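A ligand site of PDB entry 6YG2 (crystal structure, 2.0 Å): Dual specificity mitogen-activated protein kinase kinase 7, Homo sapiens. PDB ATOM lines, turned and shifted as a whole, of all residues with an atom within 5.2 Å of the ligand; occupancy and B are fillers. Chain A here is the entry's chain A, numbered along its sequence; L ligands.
SG of Cys 104 is bonded to C5 of the ligand, at 1.6 Å.
The backbone carbonyl oxygen (O) of Glu 99 sits at hydrogen-bond distance from a nitrogen (N3) of the ligand, 2.6 Å away.
The backbone NH of Met 101 is in hydrogen-bond range of a nitrogen (N1) of the ligand, at 2.8 Å.
The side-chain amino group (NZ) of Lys 107 lies within hydrogen-bond range of an oxygen (O1) of the ligand, 3.0 Å away.
The side-chain sulfur (SG) of Cys 104 is in hydrogen-bond range of the backbone NH (N) of Lys 107 (3.6 Å).
The backbone NH (N) of Lys 51 lies within hydrogen-bond range of the backbone carbonyl oxygen (O) of Ile 96 (2.8 Å).
N of Met 98 is in hydrogen-bond range of O of Ala 49 (2.7 Å).
SD of Met 28 sits close to N2 of the ligand (3.3 Å).
Residues that only touch the ligand: Gly 29 (3.8 Å), Ser 30 (3.6 Å), Gly 31 (3.2 Å), Lys 51 (3.3 Å), Ile 65 (3.2 Å), Asp 68 (3.6 Å), Leu 69 (3.5 Å), Val 82 (3.95 Å), Ile 96 (3.7 Å), Met 98 (3.5 Å), Leu 100 (3.6 Å), Glu 106 (3.8 Å), Ser 149 (3.7 Å) and Phe 164 (3.6 Å).
Hydrophobic or aromatic side chains that line the ligand: Met 28, Ile 65, Leu 69, Val 82, Ile 96, Met 98, Leu 100, Met 101 and Phe 164.
Within 4 Å of the ligand: Met 28, Gly 29, Ser 30, Gly 31, Lys 51, Ile 65, Asp 68, Leu 69, Val 82, Ile 96, Met 98, Glu 99, Leu 100, Met 101, Cys 104, Glu 106, Lys 107, Ser 149 and Phe 164.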
ATOM      1  N   MET A  28     -16.334 -34.829  -0.346  1.00  0.00           N
ATOM      2  CA  MET A  28     -17.494 -34.169  -0.910  1.00  0.00           C
ATOM      3  C   MET A  28     -17.120 -33.578  -2.264  1.00  0.00           C
ATOM      4  O   MET A  28     -17.954 -33.483  -3.172  1.00  0.00           O
ATOM      5  CB  MET A  28     -17.985 -33.089   0.032  1.00  0.00           C
ATOM      6  CG  MET A  28     -19.107 -33.505   0.976  1.00  0.00           C
ATOM      7  SD  MET A  28     -20.053 -31.982   1.244  1.00  0.00           S
ATOM      8  CE  MET A  28     -18.918 -31.018   2.211  1.00  0.00           C
ATOM      9  N   GLY A  29     -15.848 -33.223  -2.420  1.00  0.00           N
ATOM     10  CA  GLY A  29     -15.375 -32.723  -3.691  1.00  0.00           C
ATOM     11  C   GLY A  29     -14.417 -31.584  -3.471  1.00  0.00           C
ATOM     12  O   GLY A  29     -14.054 -31.267  -2.326  1.00  0.00           O
ATOM     13  N   SER A  30     -13.994 -30.956  -4.568  1.00  0.00           N
ATOM     14  CA  SER A  30     -12.998 -29.907  -4.506  1.00  0.00           C
ATOM     15  C   SER A  30     -13.568 -28.694  -3.793  1.00  0.00           C
ATOM     16  O   SER A  30     -14.224 -27.875  -4.413  1.00  0.00           O
ATOM     17  CB  SER A  30     -12.527 -29.511  -5.916  1.00  0.00           C
ATOM     18  OG  SER A  30     -13.617 -29.158  -6.753  1.00  0.00           O
ATOM     19  N   GLY A  31     -13.345 -28.626  -2.466  1.00  0.00           N
ATOM     20  CA  GLY A  31     -13.624 -27.424  -1.673  1.00  0.00           C
ATOM     21  C   GLY A  31     -12.440 -26.481  -1.550  1.00  0.00           C
ATOM     22  O   GLY A  31     -11.359 -26.730  -2.114  1.00  0.00           O
ATOM     23  N   THR A  32     -12.659 -25.367  -0.853  1.00  0.00           N
ATOM     24  CA  THR A  32     -11.553 -24.539  -0.340  1.00  0.00           C
ATOM     25  C   THR A  32     -11.410 -24.840   1.148  1.00  0.00           C
ATOM     26  O   THR A  32     -10.585 -24.243   1.835  1.00  0.00           O
ATOM     27  CB  THR A  32     -11.802 -23.038  -0.555  1.00  0.00           C
ATOM     28  N   VAL A  36     -13.786 -32.665   5.013  1.00  0.00           N
ATOM     29  CA  VAL A  36     -15.208 -32.984   4.991  1.00  0.00           C
ATOM     30  C   VAL A  36     -15.463 -34.278   4.206  1.00  0.00           C
ATOM     31  O   VAL A  36     -14.925 -34.483   3.092  1.00  0.00           O
ATOM     32  CB  VAL A  36     -16.055 -31.877   4.334  1.00  0.00           C
ATOM     33  CG1 VAL A  36     -17.533 -32.149   4.617  1.00  0.00           C
ATOM     34  CG2 VAL A  36     -15.628 -30.528   4.914  1.00  0.00           C
ATOM     35  N   ALA A  49     -22.841 -34.955   5.853  1.00  0.00           N
ATOM     36  CA  ALA A  49     -21.512 -34.434   5.694  1.00  0.00           C
ATOM     37  C   ALA A  49     -20.920 -34.253   7.026  1.00  0.00           C
ATOM     38  O   ALA A  49     -21.594 -33.746   7.948  1.00  0.00           O
ATOM     39  CB  ALA A  49     -21.546 -33.111   4.970  1.00  0.00           C
ATOM     40  N   LYS A  51     -17.637 -32.692   8.974  1.00  0.00           N
ATOM     41  CA  LYS A  51     -16.444 -31.814   8.892  1.00  0.00           C
ATOM     42  C   LYS A  51     -15.578 -32.012  10.141  1.00  0.00           C
ATOM     43  O   LYS A  51     -16.087 -32.137  11.277  1.00  0.00           O
ATOM     44  CB  LYS A  51     -16.860 -30.350   8.817  1.00  0.00           C
ATOM     45  CG  LYS A  51     -15.694 -29.391   8.957  1.00  0.00           C
ATOM     46  CD  LYS A  51     -15.939 -28.080   8.293  1.00  0.00           C
ATOM     47  CE  LYS A  51     -14.730 -27.149   8.452  1.00  0.00           C
ATOM     48  NZ  LYS A  51     -13.709 -27.337   7.374  1.00  0.00           N
ATOM     49  N   ILE A  65     -14.808 -21.317  11.764  1.00  0.00           N
ATOM     50  CA  ILE A  65     -15.617 -22.497  11.842  1.00  0.00           C
ATOM     51  C   ILE A  65     -16.618 -22.407  13.038  1.00  0.00           C
ATOM     52  O   ILE A  65     -17.795 -22.600  12.852  1.00  0.00           O
ATOM     53  CB  ILE A  65     -14.757 -23.762  11.943  1.00  0.00           C
ATOM     54  CG1 ILE A  65     -14.128 -24.070  10.567  1.00  0.00           C
ATOM     55  CG2 ILE A  65     -15.607 -24.941  12.406  1.00  0.00           C
ATOM     56  CD1 ILE A  65     -12.847 -24.906  10.625  1.00  0.00           C
ATOM     57  N   ASP A  68     -19.347 -19.784  12.409  1.00  0.00           N
ATOM     58  CA  ASP A  68     -20.318 -20.264  11.485  1.00  0.00           C
ATOM     59  C   ASP A  68     -21.162 -21.349  12.158  1.00  0.00           C
ATOM     60  O   ASP A  68     -22.339 -21.438  11.904  1.00  0.00           O
ATOM     61  CB  ASP A  68     -19.674 -20.888  10.222  1.00  0.00           C
ATOM     62  CG  ASP A  68     -18.980 -19.866   9.318  1.00  0.00           C
ATOM     63  OD1 ASP A  68     -19.243 -18.670   9.394  1.00  0.00           O
ATOM     64  OD2 ASP A  68     -18.187 -20.305   8.475  1.00  0.00           O
ATOM     65  N   LEU A  69     -20.541 -22.208  12.951  1.00  0.00           N
ATOM     66  CA  LEU A  69     -21.274 -23.256  13.667  1.00  0.00           C
ATOM     67  C   LEU A  69     -22.318 -22.663  14.616  1.00  0.00           C
ATOM     68  O   LEU A  69     -23.481 -23.125  14.664  1.00  0.00           O
ATOM     69  CB  LEU A  69     -20.321 -24.139  14.440  1.00  0.00           C
ATOM     70  CG  LEU A  69     -21.015 -25.193  15.311  1.00  0.00           C
ATOM     71  CD1 LEU A  69     -21.869 -26.131  14.475  1.00  0.00           C
ATOM     72  CD2 LEU A  69     -19.935 -25.927  16.095  1.00  0.00           C
ATOM     73  N   VAL A  72     -25.284 -21.621  12.553  1.00  0.00           N
ATOM     74  CA  VAL A  72     -26.027 -22.767  12.089  1.00  0.00           C
ATOM     75  C   VAL A  72     -26.881 -23.361  13.220  1.00  0.00           C
ATOM     76  O   VAL A  72     -28.070 -23.626  13.030  1.00  0.00           O
ATOM     77  CB  VAL A  72     -25.062 -23.817  11.495  1.00  0.00           C
ATOM     78  CG1 VAL A  72     -25.752 -25.117  11.298  1.00  0.00           C
ATOM     79  CG2 VAL A  72     -24.524 -23.313  10.169  1.00  0.00           C
ATOM     80  N   VAL A  82     -28.405 -24.581   5.823  1.00  0.00           N
ATOM     81  CA  VAL A  82     -27.961 -25.968   6.021  1.00  0.00           C
ATOM     82  C   VAL A  82     -27.927 -26.277   7.512  1.00  0.00           C
ATOM     83  O   VAL A  82     -27.378 -25.513   8.293  1.00  0.00           O
ATOM     84  CB  VAL A  82     -26.554 -26.176   5.428  1.00  0.00           C
ATOM     85  CG1 VAL A  82     -26.120 -27.611   5.546  1.00  0.00           C
ATOM     86  CG2 VAL A  82     -26.586 -25.867   3.974  1.00  0.00           C
ATOM     87  N   ILE A  96     -18.306 -32.243  13.106  1.00  0.00           N
ATOM     88  CA  ILE A  96     -19.520 -31.544  12.942  1.00  0.00           C
ATOM     89  C   ILE A  96     -20.292 -32.247  11.835  1.00  0.00           C
ATOM     90  O   ILE A  96     -19.838 -32.340  10.701  1.00  0.00           O
ATOM     91  CB  ILE A  96     -19.250 -30.059  12.522  1.00  0.00           C
ATOM     92  CG1 ILE A  96     -18.379 -29.349  13.558  1.00  0.00           C
ATOM     93  CG2 ILE A  96     -20.551 -29.340  12.334  1.00  0.00           C
ATOM     94  CD1 ILE A  96     -17.822 -28.047  13.059  1.00  0.00           C
ATOM     95  N   MET A  98     -23.394 -32.315   9.379  1.00  0.00           N
ATOM     96  CA  MET A  98     -24.231 -31.352   8.676  1.00  0.00           C
ATOM     97  C   MET A  98     -25.090 -32.030   7.668  1.00  0.00           C
ATOM     98  O   MET A  98     -24.742 -33.095   7.113  1.00  0.00           O
ATOM     99  CB  MET A  98     -23.374 -30.337   7.954  1.00  0.00           C
ATOM    100  CG  MET A  98     -22.534 -29.464   8.836  1.00  0.00           C
ATOM    101  SD  MET A  98     -23.537 -28.303   9.764  1.00  0.00           S
ATOM    102  CE  MET A  98     -23.992 -27.184   8.433  1.00  0.00           C
ATOM    103  N   GLU A  99     -26.221 -31.429   7.407  1.00  0.00           N
ATOM    104  CA  GLU A  99     -27.048 -31.777   6.270  1.00  0.00           C
ATOM    105  C   GLU A  99     -26.220 -31.762   4.985  1.00  0.00           C
ATOM    106  O   GLU A  99     -25.507 -30.779   4.697  1.00  0.00           O
ATOM    107  CB  GLU A  99     -28.173 -30.745   6.169  1.00  0.00           C
ATOM    108  CG  GLU A  99     -29.153 -30.980   5.054  1.00  0.00           C
ATOM    109  CD  GLU A  99     -30.342 -29.995   5.155  1.00  0.00           C
ATOM    110  OE1 GLU A  99     -30.176 -28.905   5.755  1.00  0.00           O
ATOM    111  OE2 GLU A  99     -31.409 -30.338   4.656  1.00  0.00           O
ATOM    112  N   LEU A 100     -26.313 -32.836   4.216  1.00  0.00           N
ATOM    113  CA  LEU A 100     -25.571 -32.957   2.973  1.00  0.00           C
ATOM    114  C   LEU A 100     -26.458 -32.520   1.802  1.00  0.00           C
ATOM    115  O   LEU A 100     -27.465 -33.147   1.514  1.00  0.00           O
ATOM    116  CB  LEU A 100     -25.148 -34.409   2.730  1.00  0.00           C
ATOM    117  CG  LEU A 100     -24.398 -34.663   1.406  1.00  0.00           C
ATOM    118  CD1 LEU A 100     -23.012 -34.032   1.433  1.00  0.00           C
ATOM    119  CD2 LEU A 100     -24.270 -36.146   1.117  1.00  0.00           C
ATOM    120  N   MET A 101     -26.049 -31.478   1.103  1.00  0.00           N
ATOM    121  CA  MET A 101     -26.714 -31.064  -0.119  1.00  0.00           C
ATOM    122  C   MET A 101     -26.036 -31.730  -1.313  1.00  0.00           C
ATOM    123  O   MET A 101     -24.986 -32.392  -1.155  1.00  0.00           O
ATOM    124  CB  MET A 101     -26.649 -29.547  -0.246  1.00  0.00           C
ATOM    125  CG  MET A 101     -27.168 -28.805   0.959  1.00  0.00           C
ATOM    126  SD  MET A 101     -28.948 -28.928   1.085  1.00  0.00           S
ATOM    127  CE  MET A 101     -29.544 -27.975  -0.342  1.00  0.00           C
ATOM    128  N   GLY A 102     -26.601 -31.539  -2.500  1.00  0.00           N
ATOM    129  CA  GLY A 102     -26.110 -32.195  -3.709  1.00  0.00           C
ATOM    130  C   GLY A 102     -24.905 -31.508  -4.272  1.00  0.00           C
ATOM    131  O   GLY A 102     -23.833 -32.158  -4.399  1.00  0.00           O
ATOM    132  N   THR A 103     -25.040 -30.208  -4.595  1.00  0.00           N
ATOM    133  CA  THR A 103     -23.915 -29.439  -5.112  1.00  0.00           C
ATOM    134  C   THR A 103     -24.308 -27.964  -5.121  1.00  0.00           C
ATOM    135  O   THR A 103     -25.413 -27.615  -4.749  1.00  0.00           O
ATOM    136  CB  THR A 103     -23.470 -29.917  -6.529  1.00  0.00           C
ATOM    137  OG1 THR A 103     -22.152 -29.456  -6.833  1.00  0.00           O
ATOM    138  CG2 THR A 103     -24.473 -29.485  -7.640  1.00  0.00           C
ATOM    139  N   CYS A 104     -23.366 -27.122  -5.513  1.00  0.00           N
ATOM    140  CA  CYS A 104     -23.587 -25.696  -5.515  1.00  0.00           C
ATOM    141  C   CYS A 104     -23.942 -25.198  -6.908  1.00  0.00           C
ATOM    142  O   CYS A 104     -23.722 -25.894  -7.958  1.00  0.00           O
ATOM    143  CB  CYS A 104     -22.346 -25.022  -4.985  1.00  0.00           C
ATOM    144  SG  CYS A 104     -20.929 -25.250  -6.037  1.00  0.00           S
ATOM    145  N   GLU A 106     -22.610 -22.887  -8.628  1.00  0.00           N
ATOM    146  CA  GLU A 106     -21.414 -22.740  -9.445  1.00  0.00           C
ATOM    147  C   GLU A 106     -21.155 -24.034 -10.276  1.00  0.00           C
ATOM    148  O   GLU A 106     -20.855 -23.978 -11.476  1.00  0.00           O
ATOM    149  CB  GLU A 106     -20.198 -22.460  -8.571  1.00  0.00           C
ATOM    150  CG  GLU A 106     -18.947 -22.263  -9.388  1.00  0.00           C
ATOM    151  CD  GLU A 106     -17.680 -22.630  -8.663  1.00  0.00           C
ATOM    152  OE1 GLU A 106     -17.738 -23.166  -7.522  1.00  0.00           O
ATOM    153  OE2 GLU A 106     -16.598 -22.392  -9.247  1.00  0.00           O
ATOM    154  N   LYS A 107     -21.266 -25.162  -9.598  1.00  0.00           N
ATOM    155  CA  LYS A 107     -21.006 -26.474 -10.228  1.00  0.00           C
ATOM    156  C   LYS A 107     -22.136 -26.882 -11.134  1.00  0.00           C
ATOM    157  O   LYS A 107     -21.890 -27.477 -12.175  1.00  0.00           O
ATOM    158  CB  LYS A 107     -20.643 -27.544  -9.195  1.00  0.00           C
ATOM    159  CG  LYS A 107     -19.227 -27.325  -8.698  1.00  0.00           C
ATOM    160  CD  LYS A 107     -18.887 -28.287  -7.564  1.00  0.00           C
ATOM    161  CE  LYS A 107     -17.391 -28.307  -7.253  1.00  0.00           C
ATOM    162  NZ  LYS A 107     -17.131 -29.086  -5.996  1.00  0.00           N
ATOM    163  N   SER A 149     -21.257 -20.181  -5.783  1.00  0.00           N
ATOM    164  CA  SER A 149     -20.650 -21.237  -4.994  1.00  0.00           C
ATOM    165  C   SER A 149     -21.243 -21.378  -3.588  1.00  0.00           C
ATOM    166  O   SER A 149     -21.050 -22.418  -2.988  1.00  0.00           O
ATOM    167  CB  SER A 149     -19.121 -21.081  -4.928  1.00  0.00           C
ATOM    168  OG  SER A 149     -18.801 -19.859  -4.328  1.00  0.00           O
ATOM    169  N   LEU A 152     -26.617 -23.735  -2.556  1.00  0.00           N
ATOM    170  CA  LEU A 152     -26.630 -25.200  -2.648  1.00  0.00           C
ATOM    171  C   LEU A 152     -27.998 -25.719  -2.983  1.00  0.00           C
ATOM    172  O   LEU A 152     -28.987 -25.190  -2.526  1.00  0.00           O
ATOM    173  CB  LEU A 152     -26.192 -25.807  -1.318  1.00  0.00           C
ATOM    174  CG  LEU A 152     -24.808 -25.398  -0.823  1.00  0.00           C
ATOM    175  CD1 LEU A 152     -24.500 -26.192   0.447  1.00  0.00           C
ATOM    176  CD2 LEU A 152     -23.721 -25.654  -1.856  1.00  0.00           C
ATOM    177  N   CYS A 162     -25.026 -20.855   1.957  1.00  0.00           N
ATOM    178  CA  CYS A 162     -23.772 -21.381   2.484  1.00  0.00           C
ATOM    179  C   CYS A 162     -22.810 -20.211   2.812  1.00  0.00           C
ATOM    180  O   CYS A 162     -23.000 -19.099   2.355  1.00  0.00           O
ATOM    181  CB  CYS A 162     -23.127 -22.277   1.435  1.00  0.00           C
ATOM    182  SG  CYS A 162     -22.163 -23.631   2.106  1.00  0.00           S
ATOM    183  N   PHE A 164     -19.450 -21.383   4.500  1.00  0.00           N
ATOM    184  CA  PHE A 164     -18.243 -22.045   4.960  1.00  0.00           C
ATOM    185  C   PHE A 164     -17.324 -22.335   3.778  1.00  0.00           C
ATOM    186  O   PHE A 164     -16.571 -21.473   3.336  1.00  0.00           O
ATOM    187  CB  PHE A 164     -18.585 -23.331   5.704  1.00  0.00           C
HETATM  188  N1  LIG L   1     -23.489 -30.330   1.562  1.00  0.00           N
HETATM  189  C1  LIG L   1     -23.016 -30.281   0.298  1.00  0.00           C
HETATM  190  N2  LIG L   1     -21.961 -29.627  -0.174  1.00  0.00           N
HETATM  191  C2  LIG L   1     -21.313 -28.977   0.804  1.00  0.00           C
HETATM  192  C3  LIG L   1     -21.668 -28.947   2.176  1.00  0.00           C
HETATM  193  C4  LIG L   1     -22.825 -29.654   2.521  1.00  0.00           C
HETATM  194  C5  LIG L   1     -19.680 -25.242  -5.026  1.00  0.00           C
HETATM  195  N3  LIG L   1     -23.289 -29.718   3.763  1.00  0.00           N
HETATM  196  O1  LIG L   1     -17.596 -26.662  -4.239  1.00  0.00           O
HETATM  197  C6  LIG L   1     -19.763 -26.014  -3.652  1.00  0.00           C
HETATM  198  C7  LIG L   1     -19.162 -24.413  10.550  1.00  0.00           C
HETATM  199  C8  LIG L   1     -18.198 -24.633   9.584  1.00  0.00           C
HETATM  200  C9  LIG L   1     -20.178 -25.303  10.726  1.00  0.00           C
HETATM  201  C10 LIG L   1     -18.249 -25.775   8.799  1.00  0.00           C
HETATM  202  C11 LIG L   1     -20.243 -26.452   9.966  1.00  0.00           C
HETATM  203  C12 LIG L   1     -19.485 -26.821   6.117  1.00  0.00           C
HETATM  204  C13 LIG L   1     -19.974 -29.157   6.404  1.00  0.00           C
HETATM  205  C14 LIG L   1     -19.897 -26.905   4.790  1.00  0.00           C
HETATM  206  C15 LIG L   1     -20.364 -29.233   5.082  1.00  0.00           C
HETATM  207  C16 LIG L   1     -17.044 -29.084  -1.417  1.00  0.00           C
HETATM  208  C17 LIG L   1     -17.983 -29.099  -0.224  1.00  0.00           C
HETATM  209  C18 LIG L   1     -16.831 -27.672  -1.867  1.00  0.00           C
HETATM  210  C19 LIG L   1     -18.953 -26.916  -0.908  1.00  0.00           C
HETATM  211  N4  LIG L   1     -19.716 -27.816   1.906  1.00  0.00           N
HETATM  212  O2  LIG L   1     -19.326 -27.894   8.303  1.00  0.00           O
HETATM  213  C20 LIG L   1     -18.418 -26.601  -3.351  1.00  0.00           C
HETATM  214  C21 LIG L   1     -19.272 -26.693   8.999  1.00  0.00           C
HETATM  215  C22 LIG L   1     -19.541 -27.947   6.925  1.00  0.00           C
HETATM  216  C23 LIG L   1     -20.338 -28.104   4.267  1.00  0.00           C
HETATM  217  C24 LIG L   1     -20.610 -28.233   2.797  1.00  0.00           C
HETATM  218  C25 LIG L   1     -19.280 -28.332  -0.504  1.00  0.00           C
HETATM  219  N5  LIG L   1     -20.141 -28.317   0.684  1.00  0.00           N
HETATM  220  N6  LIG L   1     -18.127 -27.011  -2.105  1.00  0.00           N
